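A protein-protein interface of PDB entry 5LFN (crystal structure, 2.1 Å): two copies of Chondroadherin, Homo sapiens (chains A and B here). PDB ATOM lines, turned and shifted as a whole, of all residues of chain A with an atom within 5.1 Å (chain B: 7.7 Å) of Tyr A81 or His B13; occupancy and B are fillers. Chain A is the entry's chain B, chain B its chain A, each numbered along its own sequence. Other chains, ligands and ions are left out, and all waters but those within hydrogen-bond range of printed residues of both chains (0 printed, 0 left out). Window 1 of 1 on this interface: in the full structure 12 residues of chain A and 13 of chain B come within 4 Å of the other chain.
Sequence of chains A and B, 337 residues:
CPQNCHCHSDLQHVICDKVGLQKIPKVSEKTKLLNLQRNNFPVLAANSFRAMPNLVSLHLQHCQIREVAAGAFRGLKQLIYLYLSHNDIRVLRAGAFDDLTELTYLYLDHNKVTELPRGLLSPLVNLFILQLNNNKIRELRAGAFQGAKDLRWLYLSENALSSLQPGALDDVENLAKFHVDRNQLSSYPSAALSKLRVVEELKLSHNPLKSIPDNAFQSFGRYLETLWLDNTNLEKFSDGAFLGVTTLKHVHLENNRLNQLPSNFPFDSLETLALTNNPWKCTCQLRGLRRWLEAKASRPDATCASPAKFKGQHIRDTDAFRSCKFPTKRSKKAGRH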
ATOM      1  N   VAL A  56     -14.517  -5.407  -0.357  1.00  0.00           N
ATOM      2  CA  VAL A  56     -14.195  -6.816  -0.217  1.00  0.00           C
ATOM      3  C   VAL A  56     -13.091  -7.060   0.808  1.00  0.00           C
ATOM      4  O   VAL A  56     -13.080  -8.121   1.443  1.00  0.00           O
ATOM      5  CB  VAL A  56     -13.812  -7.421  -1.584  1.00  0.00           C
ATOM      6  CG1 VAL A  56     -13.299  -8.849  -1.429  1.00  0.00           C
ATOM      7  CG2 VAL A  56     -15.001  -7.385  -2.532  1.00  0.00           C
ATOM      8  N   SER A  57     -12.174  -6.114   0.993  1.00  0.00           N
ATOM      9  CA  SER A  57     -11.043  -6.286   1.892  1.00  0.00           C
ATOM     10  C   SER A  57     -10.840  -5.006   2.690  1.00  0.00           C
ATOM     11  O   SER A  57     -10.929  -3.903   2.141  1.00  0.00           O
ATOM     12  CB  SER A  57      -9.768  -6.637   1.113  1.00  0.00           C
ATOM     13  OG  SER A  57      -8.668  -6.824   1.985  1.00  0.00           O
ATOM     14  N   LEU A  58     -10.568  -5.161   3.985  1.00  0.00           N
ATOM     15  CA  LEU A  58     -10.451  -4.031   4.902  1.00  0.00           C
ATOM     16  C   LEU A  58      -9.281  -4.276   5.841  1.00  0.00           C
ATOM     17  O   LEU A  58      -9.284  -5.254   6.595  1.00  0.00           O
ATOM     18  CB  LEU A  58     -11.748  -3.835   5.694  1.00  0.00           C
ATOM     19  CG  LEU A  58     -11.756  -2.740   6.761  1.00  0.00           C
ATOM     20  CD1 LEU A  58     -11.394  -1.388   6.167  1.00  0.00           C
ATOM     21  CD2 LEU A  58     -13.118  -2.683   7.439  1.00  0.00           C
ATOM     22  N   LEU A  79     -18.045  -7.868   2.520  1.00  0.00           N
ATOM     23  CA  LEU A  79     -16.692  -7.966   3.047  1.00  0.00           C
ATOM     24  C   LEU A  79     -16.262  -9.424   3.149  1.00  0.00           C
ATOM     25  O   LEU A  79     -17.011 -10.272   3.644  1.00  0.00           O
ATOM     26  CB  LEU A  79     -16.601  -7.294   4.416  1.00  0.00           C
ATOM     27  CG  LEU A  79     -15.183  -7.007   4.917  1.00  0.00           C
ATOM     28  CD1 LEU A  79     -14.511  -5.930   4.073  1.00  0.00           C
ATOM     29  CD2 LEU A  79     -15.192  -6.610   6.385  1.00  0.00           C
ATOM     30  N   ILE A  80     -15.053  -9.711   2.674  1.00  0.00           N
ATOM     31  CA  ILE A  80     -14.482 -11.046   2.723  1.00  0.00           C
ATOM     32  C   ILE A  80     -13.339 -11.128   3.729  1.00  0.00           C
ATOM     33  O   ILE A  80     -13.265 -12.078   4.511  1.00  0.00           O
ATOM     34  CB  ILE A  80     -14.015 -11.486   1.318  1.00  0.00           C
ATOM     35  CG1 ILE A  80     -15.181 -11.431   0.321  1.00  0.00           C
ATOM     36  CG2 ILE A  80     -13.395 -12.881   1.357  1.00  0.00           C
ATOM     37  CD1 ILE A  80     -16.343 -12.356   0.646  1.00  0.00           C
ATOM     38  N   TYR A  81     -12.443 -10.145   3.721  1.00  0.00           N
ATOM     39  CA  TYR A  81     -11.302 -10.104   4.624  1.00  0.00           C
ATOM     40  C   TYR A  81     -11.500  -8.983   5.634  1.00  0.00           C
ATOM     41  O   TYR A  81     -11.993  -7.905   5.287  1.00  0.00           O
ATOM     42  CB  TYR A  81      -9.998  -9.861   3.859  1.00  0.00           C
ATOM     43  CG  TYR A  81      -9.688 -10.887   2.795  1.00  0.00           C
ATOM     44  CD1 TYR A  81     -10.352 -10.866   1.576  1.00  0.00           C
ATOM     45  CD2 TYR A  81      -8.721 -11.865   2.997  1.00  0.00           C
ATOM     46  CE1 TYR A  81     -10.073 -11.791   0.595  1.00  0.00           C
ATOM     47  CE2 TYR A  81      -8.435 -12.796   2.018  1.00  0.00           C
ATOM     48  CZ  TYR A  81      -9.115 -12.754   0.819  1.00  0.00           C
ATOM     49  OH  TYR A  81      -8.841 -13.676  -0.164  1.00  0.00           O
ATOM     50  N   LEU A  82     -11.106  -9.231   6.882  1.00  0.00           N
ATOM     51  CA  LEU A  82     -11.086  -8.189   7.905  1.00  0.00           C
ATOM     52  C   LEU A  82      -9.841  -8.390   8.756  1.00  0.00           C
ATOM     53  O   LEU A  82      -9.725  -9.400   9.457  1.00  0.00           O
ATOM     54  CB  LEU A  82     -12.354  -8.223   8.762  1.00  0.00           C
ATOM     55  CG  LEU A  82     -12.398  -7.244   9.939  1.00  0.00           C
ATOM     56  CD1 LEU A  82     -12.112  -5.824   9.479  1.00  0.00           C
ATOM     57  CD2 LEU A  82     -13.747  -7.317  10.641  1.00  0.00           C
ATOM     58  N   TYR A  83      -8.917  -7.432   8.698  1.00  0.00           N
ATOM     59  CA  TYR A  83      -7.668  -7.489   9.447  1.00  0.00           C
ATOM     60  C   TYR A  83      -7.732  -6.492  10.596  1.00  0.00           C
ATOM     61  O   TYR A  83      -7.804  -5.281  10.367  1.00  0.00           O
ATOM     62  CB  TYR A  83      -6.474  -7.184   8.543  1.00  0.00           C
ATOM     63  CG  TYR A  83      -6.316  -8.150   7.392  1.00  0.00           C
ATOM     64  CD1 TYR A  83      -6.924  -7.907   6.167  1.00  0.00           C
ATOM     65  CD2 TYR A  83      -5.558  -9.306   7.530  1.00  0.00           C
ATOM     66  CE1 TYR A  83      -6.779  -8.787   5.112  1.00  0.00           C
ATOM     67  CE2 TYR A  83      -5.410 -10.192   6.480  1.00  0.00           C
ATOM     68  CZ  TYR A  83      -6.023  -9.928   5.274  1.00  0.00           C
ATOM     69  OH  TYR A  83      -5.879 -10.807   4.226  1.00  0.00           O
ATOM     70  N   LEU A 103     -18.138 -12.588   5.406  1.00  0.00           N
ATOM     71  CA  LEU A 103     -16.802 -12.579   5.985  1.00  0.00           C
ATOM     72  C   LEU A 103     -16.248 -13.996   6.053  1.00  0.00           C
ATOM     73  O   LEU A 103     -16.881 -14.899   6.609  1.00  0.00           O
ATOM     74  CB  LEU A 103     -16.822 -11.958   7.380  1.00  0.00           C
ATOM     75  CG  LEU A 103     -15.430 -11.702   7.967  1.00  0.00           C
ATOM     76  CD1 LEU A 103     -14.761 -10.544   7.243  1.00  0.00           C
ATOM     77  CD2 LEU A 103     -15.486 -11.443   9.463  1.00  0.00           C
ATOM     78  N   TYR A 105     -12.409 -14.471   6.384  1.00  0.00           N
ATOM     79  CA  TYR A 105     -11.145 -14.463   7.109  1.00  0.00           C
ATOM     80  C   TYR A 105     -11.162 -13.308   8.095  1.00  0.00           C
ATOM     81  O   TYR A 105     -11.372 -12.156   7.702  1.00  0.00           O
ATOM     82  CB  TYR A 105      -9.968 -14.329   6.142  1.00  0.00           C
ATOM     83  CG  TYR A 105     -10.154 -15.157   4.895  1.00  0.00           C
ATOM     84  CD1 TYR A 105      -9.777 -16.491   4.856  1.00  0.00           C
ATOM     85  CD2 TYR A 105     -10.723 -14.603   3.757  1.00  0.00           C
ATOM     86  CE1 TYR A 105      -9.957 -17.249   3.715  1.00  0.00           C
ATOM     87  CE2 TYR A 105     -10.905 -15.347   2.614  1.00  0.00           C
ATOM     88  CZ  TYR A 105     -10.525 -16.671   2.597  1.00  0.00           C
ATOM     89  OH  TYR A 105     -10.708 -17.408   1.450  1.00  0.00           O
ATOM     90  N   CYS B   1      -6.937 -26.051  -6.060  1.00  0.00           N
ATOM     91  CA  CYS B   1      -6.494 -25.440  -4.814  1.00  0.00           C
ATOM     92  C   CYS B   1      -5.470 -26.343  -4.123  1.00  0.00           C
ATOM     93  O   CYS B   1      -5.784 -27.486  -3.802  1.00  0.00           O
ATOM     94  CB  CYS B   1      -7.682 -25.190  -3.889  1.00  0.00           C
ATOM     95  SG  CYS B   1      -7.351 -24.013  -2.568  1.00  0.00           S
ATOM     96  N   PRO B   2      -4.252 -25.848  -3.890  1.00  0.00           N
ATOM     97  CA  PRO B   2      -3.221 -26.710  -3.298  1.00  0.00           C
ATOM     98  C   PRO B   2      -3.577 -27.145  -1.884  1.00  0.00           C
ATOM     99  O   PRO B   2      -4.363 -26.507  -1.180  1.00  0.00           O
ATOM    100  CB  PRO B   2      -1.965 -25.828  -3.297  1.00  0.00           C
ATOM    101  CG  PRO B   2      -2.284 -24.657  -4.160  1.00  0.00           C
ATOM    102  CD  PRO B   2      -3.757 -24.476  -4.095  1.00  0.00           C
ATOM    103  N   CYS B   5      -3.530 -25.031   1.655  1.00  0.00           N
ATOM    104  CA  CYS B   5      -3.962 -23.684   1.312  1.00  0.00           C
ATOM    105  C   CYS B   5      -5.472 -23.660   1.094  1.00  0.00           C
ATOM    106  O   CYS B   5      -6.093 -24.682   0.789  1.00  0.00           O
ATOM    107  CB  CYS B   5      -3.234 -23.177   0.064  1.00  0.00           C
ATOM    108  SG  CYS B   5      -1.425 -23.196   0.196  1.00  0.00           S
ATOM    109  N   HIS B   6      -6.060 -22.475   1.254  1.00  0.00           N
ATOM    110  CA  HIS B   6      -7.486 -22.274   1.039  1.00  0.00           C
ATOM    111  C   HIS B   6      -7.713 -21.278  -0.093  1.00  0.00           C
ATOM    112  O   HIS B   6      -6.940 -20.332  -0.275  1.00  0.00           O
ATOM    113  CB  HIS B   6      -8.188 -21.783   2.304  1.00  0.00           C
ATOM    114  CG  HIS B   6      -9.665 -21.606   2.133  1.00  0.00           C
ATOM    115  ND1 HIS B   6     -10.267 -20.369   2.076  1.00  0.00           N
ATOM    116  CD2 HIS B   6     -10.657 -22.516   1.987  1.00  0.00           C
ATOM    117  CE1 HIS B   6     -11.569 -20.523   1.911  1.00  0.00           C
ATOM    118  NE2 HIS B   6     -11.833 -21.816   1.855  1.00  0.00           N
ATOM    119  N   CYS B   7      -8.782 -21.507  -0.854  1.00  0.00           N
ATOM    120  CA  CYS B   7      -9.098 -20.719  -2.038  1.00  0.00           C
ATOM    121  C   CYS B   7     -10.526 -20.193  -1.965  1.00  0.00           C
ATOM    122  O   CYS B   7     -11.452 -20.928  -1.612  1.00  0.00           O
ATOM    123  CB  CYS B   7      -8.924 -21.554  -3.307  1.00  0.00           C
ATOM    124  SG  CYS B   7      -7.262 -22.218  -3.515  1.00  0.00           S
ATOM    125  N   HIS B   8     -10.694 -18.914  -2.299  1.00  0.00           N
ATOM    126  CA  HIS B   8     -12.010 -18.297  -2.417  1.00  0.00           C
ATOM    127  C   HIS B   8     -12.476 -18.430  -3.863  1.00  0.00           C
ATOM    128  O   HIS B   8     -11.789 -17.981  -4.785  1.00  0.00           O
ATOM    129  CB  HIS B   8     -11.984 -16.830  -1.992  1.00  0.00           C
ATOM    130  CG  HIS B   8     -13.317 -16.315  -1.545  1.00  0.00           C
ATOM    131  ND1 HIS B   8     -14.272 -15.860  -2.428  1.00  0.00           N
ATOM    132  CD2 HIS B   8     -13.858 -16.188  -0.310  1.00  0.00           C
ATOM    133  CE1 HIS B   8     -15.344 -15.475  -1.757  1.00  0.00           C
ATOM    134  NE2 HIS B   8     -15.117 -15.663  -0.469  1.00  0.00           N
ATOM    135  N   SER B   9     -13.642 -19.052  -4.054  1.00  0.00           N
ATOM    136  CA  SER B   9     -14.073 -19.445  -5.392  1.00  0.00           C
ATOM    137  C   SER B   9     -14.158 -18.248  -6.334  1.00  0.00           C
ATOM    138  O   SER B   9     -13.489 -18.209  -7.372  1.00  0.00           O
ATOM    139  CB  SER B   9     -15.432 -20.144  -5.300  1.00  0.00           C
ATOM    140  OG  SER B   9     -15.385 -21.256  -4.424  1.00  0.00           O
ATOM    141  N   ASP B  10     -14.979 -17.258  -5.984  1.00  0.00           N
ATOM    142  CA  ASP B  10     -15.254 -16.162  -6.910  1.00  0.00           C
ATOM    143  C   ASP B  10     -14.027 -15.287  -7.145  1.00  0.00           C
ATOM    144  O   ASP B  10     -13.811 -14.801  -8.261  1.00  0.00           O
ATOM    145  CB  ASP B  10     -16.416 -15.312  -6.396  1.00  0.00           C
ATOM    146  CG  ASP B  10     -16.818 -14.227  -7.377  1.00  0.00           C
ATOM    147  OD1 ASP B  10     -17.437 -14.559  -8.410  1.00  0.00           O
ATOM    148  OD2 ASP B  10     -16.513 -13.044  -7.119  1.00  0.00           O
ATOM    149  N   LEU B  11     -13.209 -15.079  -6.113  1.00  0.00           N
ATOM    150  CA  LEU B  11     -12.152 -14.077  -6.174  1.00  0.00           C
ATOM    151  C   LEU B  11     -10.860 -14.563  -6.822  1.00  0.00           C
ATOM    152  O   LEU B  11     -10.014 -13.726  -7.156  1.00  0.00           O
ATOM    153  CB  LEU B  11     -11.835 -13.590  -4.757  1.00  0.00           C
ATOM    154  CG  LEU B  11     -13.001 -13.010  -3.954  1.00  0.00           C
ATOM    155  CD1 LEU B  11     -12.550 -12.687  -2.537  1.00  0.00           C
ATOM    156  CD2 LEU B  11     -13.576 -11.775  -4.628  1.00  0.00           C
ATOM    157  N   GLN B  12     -10.678 -15.868  -7.018  1.00  0.00           N
ATOM    158  CA  GLN B  12      -9.420 -16.398  -7.549  1.00  0.00           C
ATOM    159  C   GLN B  12      -8.243 -16.017  -6.653  1.00  0.00           C
ATOM    160  O   GLN B  12      -7.167 -15.648  -7.128  1.00  0.00           O
ATOM    161  CB  GLN B  12      -9.179 -15.930  -8.988  1.00  0.00           C
ATOM    162  CG  GLN B  12      -9.997 -16.675 -10.026  1.00  0.00           C
ATOM    163  CD  GLN B  12      -9.618 -18.141 -10.106  1.00  0.00           C
ATOM    164  OE1 GLN B  12      -8.530 -18.534  -9.683  1.00  0.00           O
ATOM    165  NE2 GLN B  12     -10.513 -18.958 -10.645  1.00  0.00           N
ATOM    166  N   HIS B  13      -8.452 -16.110  -5.344  1.00  0.00           N
ATOM    167  CA  HIS B  13      -7.415 -15.855  -4.356  1.00  0.00           C
ATOM    168  C   HIS B  13      -6.877 -17.175  -3.821  1.00  0.00           C
ATOM    169  O   HIS B  13      -7.632 -18.134  -3.634  1.00  0.00           O
ATOM    170  CB  HIS B  13      -7.956 -15.004  -3.205  1.00  0.00           C
ATOM    171  CG  HIS B  13      -8.292 -13.598  -3.597  1.00  0.00           C
ATOM    172  ND1 HIS B  13      -8.521 -12.601  -2.672  1.00  0.00           N
ATOM    173  CD2 HIS B  13      -8.430 -13.021  -4.814  1.00  0.00           C
ATOM    174  CE1 HIS B  13      -8.793 -11.473  -3.303  1.00  0.00           C
ATOM    175  NE2 HIS B  13      -8.744 -11.701  -4.603  1.00  0.00           N
ATOM    176  N   VAL B  14      -5.569 -17.221  -3.583  1.00  0.00           N
ATOM    177  CA  VAL B  14      -4.914 -18.378  -2.983  1.00  0.00           C
ATOM    178  C   VAL B  14      -4.273 -17.916  -1.682  1.00  0.00           C
ATOM    179  O   VAL B  14      -3.455 -16.989  -1.680  1.00  0.00           O
ATOM    180  CB  VAL B  14      -3.868 -18.998  -3.925  1.00  0.00           C
ATOM    181  CG1 VAL B  14      -3.139 -20.148  -3.239  1.00  0.00           C
ATOM    182  CG2 VAL B  14      -4.526 -19.485  -5.208  1.00  0.00           C
ATOM    183  N   ILE B  15      -4.643 -18.567  -0.584  1.00  0.00           N
ATOM    184  CA  ILE B  15      -4.182 -18.206   0.752  1.00  0.00           C
ATOM    185  C   ILE B  15      -3.367 -19.369   1.296  1.00  0.00           C
ATOM    186  O   ILE B  15      -3.900 -20.466   1.506  1.00  0.00           O
ATOM    187  CB  ILE B  15      -5.358 -17.869   1.684  1.00  0.00           C
ATOM    188  CG1 ILE B  15      -6.166 -16.707   1.099  1.00  0.00           C
ATOM    189  CG2 ILE B  15      -4.860 -17.543   3.092  1.00  0.00           C
ATOM    190  CD1 ILE B  15      -7.427 -16.395   1.857  1.00  0.00           C
ATOM    191  N   CYS B  16      -2.080 -19.127   1.525  1.00  0.00           N
ATOM    192  CA  CYS B  16      -1.166 -20.110   2.089  1.00  0.00           C
ATOM    193  C   CYS B  16      -0.460 -19.530   3.305  1.00  0.00           C
ATOM    194  O   CYS B  16       0.730 -19.770   3.531  1.00  0.00           O
ATOM    195  CB  CYS B  16      -0.147 -20.568   1.047  1.00  0.00           C
ATOM    196  SG  CYS B  16      -0.846 -21.351  -0.433  1.00  0.00           S
ATOM    197  N   LYS B  30      -5.471 -18.541 -13.698  1.00  0.00           N
ATOM    198  CA  LYS B  30      -6.273 -17.353 -13.431  1.00  0.00           C
ATOM    199  C   LYS B  30      -6.045 -16.769 -12.045  1.00  0.00           C
ATOM    200  O   LYS B  30      -6.650 -15.738 -11.728  1.00  0.00           O
ATOM    201  CB  LYS B  30      -7.764 -17.650 -13.598  1.00  0.00           C
ATOM    202  CG  LYS B  30      -8.213 -17.871 -15.030  1.00  0.00           C
ATOM    203  CD  LYS B  30      -9.693 -18.207 -15.077  1.00  0.00           C
ATOM    204  CE  LYS B  30     -10.535 -16.947 -14.906  1.00  0.00           C
ATOM    205  NZ  LYS B  30     -11.990 -17.194 -15.089  1.00  0.00           N
ATOM    206  N   THR B  31      -5.216 -17.391 -11.210  1.00  0.00           N
ATOM    207  CA  THR B  31      -4.985 -16.865  -9.872  1.00  0.00           C
ATOM    208  C   THR B  31      -4.590 -15.397  -9.953  1.00  0.00           C
ATOM    209  O   THR B  31      -3.669 -15.025 -10.686  1.00  0.00           O
ATOM    210  CB  THR B  31      -3.896 -17.675  -9.163  1.00  0.00           C
ATOM    211  OG1 THR B  31      -4.291 -19.048  -9.083  1.00  0.00           O
ATOM    212  CG2 THR B  31      -3.661 -17.144  -7.752  1.00  0.00           C
ATOM    213  N   LYS B  32      -5.299 -14.565  -9.188  1.00  0.00           N
ATOM    214  CA  LYS B  32      -5.061 -13.130  -9.163  1.00  0.00           C
ATOM    215  C   LYS B  32      -4.389 -12.652  -7.888  1.00  0.00           C
ATOM    216  O   LYS B  32      -3.801 -11.566  -7.890  1.00  0.00           O
ATOM    217  CB  LYS B  32      -6.389 -12.379  -9.344  1.00  0.00           C
ATOM    218  CG  LYS B  32      -7.009 -12.576 -10.722  1.00  0.00           C
ATOM    219  CD  LYS B  32      -8.344 -11.862 -10.862  1.00  0.00           C
ATOM    220  CE  LYS B  32      -8.180 -10.356 -10.952  1.00  0.00           C
ATOM    221  NZ  LYS B  32      -9.491  -9.680 -11.151  1.00  0.00           N
ATOM    222  N   LEU B  33      -4.461 -13.428  -6.809  1.00  0.00           N
ATOM    223  CA  LEU B  33      -3.797 -13.097  -5.558  1.00  0.00           C
ATOM    224  C   LEU B  33      -3.197 -14.369  -4.986  1.00  0.00           C
ATOM    225  O   LEU B  33      -3.870 -15.402  -4.924  1.00  0.00           O
ATOM    226  CB  LEU B  33      -4.773 -12.474  -4.552  1.00  0.00           C
ATOM    227  CG  LEU B  33      -4.167 -11.919  -3.259  1.00  0.00           C
ATOM    228  CD1 LEU B  33      -5.014 -10.764  -2.734  1.00  0.00           C
ATOM    229  CD2 LEU B  33      -4.032 -12.995  -2.186  1.00  0.00           C
ATOM    230  N   LEU B  34      -1.934 -14.291  -4.573  1.00  0.00           N
ATOM    231  CA  LEU B  34      -1.223 -15.429  -4.000  1.00  0.00           C
ATOM    232  C   LEU B  34      -0.566 -14.964  -2.709  1.00  0.00           C
ATOM    233  O   LEU B  34       0.368 -14.157  -2.739  1.00  0.00           O
ATOM    234  CB  LEU B  34      -0.188 -15.986  -4.978  1.00  0.00           C
ATOM    235  CG  LEU B  34       0.556 -17.245  -4.532  1.00  0.00           C
ATOM    236  CD1 LEU B  34      -0.406 -18.413  -4.355  1.00  0.00           C
ATOM    237  CD2 LEU B  34       1.647 -17.594  -5.525  1.00  0.00           C
ATOM    238  N   ASN B  35      -1.062 -15.463  -1.579  1.00  0.00           N
ATOM    239  CA  ASN B  35      -0.559 -15.089  -0.263  1.00  0.00           C
ATOM    240  C   ASN B  35       0.289 -16.238   0.271  1.00  0.00           C
ATOM    241  O   ASN B  35      -0.244 -17.285   0.655  1.00  0.00           O
ATOM    242  CB  ASN B  35      -1.716 -14.768   0.681  1.00  0.00           C
ATOM    243  CG  ASN B  35      -1.249 -14.277   2.037  1.00  0.00           C
ATOM    244  OD1 ASN B  35      -0.079 -14.414   2.393  1.00  0.00           O
ATOM    245  ND2 ASN B  35      -2.167 -13.697   2.804  1.00  0.00           N
ATOM    246  N   SER B  57      -1.402  -9.675  -7.410  1.00  0.00           N
ATOM    247  CA  SER B  57      -0.816  -9.377  -6.108  1.00  0.00           C
ATOM    248  C   SER B  57      -0.076 -10.609  -5.611  1.00  0.00           C
ATOM    249  O   SER B  57      -0.564 -11.732  -5.755  1.00  0.00           O
ATOM    250  CB  SER B  57      -1.894  -8.963  -5.098  1.00  0.00           C
ATOM    251  OG  SER B  57      -1.342  -8.659  -3.832  1.00  0.00           O
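ND1 of His B6 sits at hydrogen-bond distance from OH of Tyr A105. OH of Tyr A81 sits at hydrogen-bond distance from ND1 of His B13, at 2.7 Å.
Hydrophobic or aromatic side chains of chain B within 4 Å of the printed part of chain A: His B6, His B8, Leu B11, His B13 and Ile B15. Of the 10 printed residues of chain A, 3 touch a printed residue of chain B. Along chain A the printed residues that touch a printed residue of chain B span positions 80 to 105. Among the printed residues, 7 pairs touch across the chains.
His B8 touches Ile A80. CD1 of Leu B11 touches CG2 of Ile A80, at 3.99 Å. Ile B15 touches Tyr A81. His B8 touches Tyr A105 (CB to OH, 3.7 Å). CZ of Tyr A105 touches CD1 of Ile B15, 3.2 Å away.
1 position is printed for both chains.
Leu A58 touches none of the printed residues of chain B. Of the printed residues of chain B, Ile A80 touches His B8 (3.7 Å) and Leu B11 (3.99 Å). Printed residues of chain B within 4 Å of Tyr A81: His B13 and Ile B15. Printed residues of chain B within 4 Å of Tyr A105: His B6, His B8 and Ile B15. Pro B2 touches none of the printed residues of chain A. Of the printed residues of chain A, His B8 touches Ile A80 (3.7 Å) and Tyr A105 (3.7 Å). Of chain A, only Tyr A81 comes within 4 Å of His B13. Of the printed residues of chain A, Ile B15 touches Tyr A81 and Tyr A105. The nearest residue of chain B that does not touch Tyr A81 is Leu B11 (4.1 Å). The nearest printed residue of chain A that does not touch His B13 is Val A56 (5.5 Å). The nearest printed residue of chain A that does not touch Ile B15 is Tyr A83 (6.3 Å).
SG of Cys B16 is disulfide-bonded to SG of Cys B5 (2.0 Å). N of Leu A82 lies within hydrogen-bond range of O of Tyr A105, 3.0 Å away. The backbone NH (N) of Ile B15 lies within hydrogen-bond range of the backbone carbonyl oxygen (O) of His B6. The backbone carbonyl oxygen (O) of Ile A80 is in hydrogen-bond range of the backbone NH (N) of Tyr A105 (3.2 Å). The side-chain sulfur (SG) of Cys B7 forms a disulfide with the side-chain sulfur (SG) of Cys B1 (2.0 Å). The backbone NH (N) of His B8 sits at hydrogen-bond distance from the backbone carbonyl oxygen (O) of His B13, 3.4 Å away.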
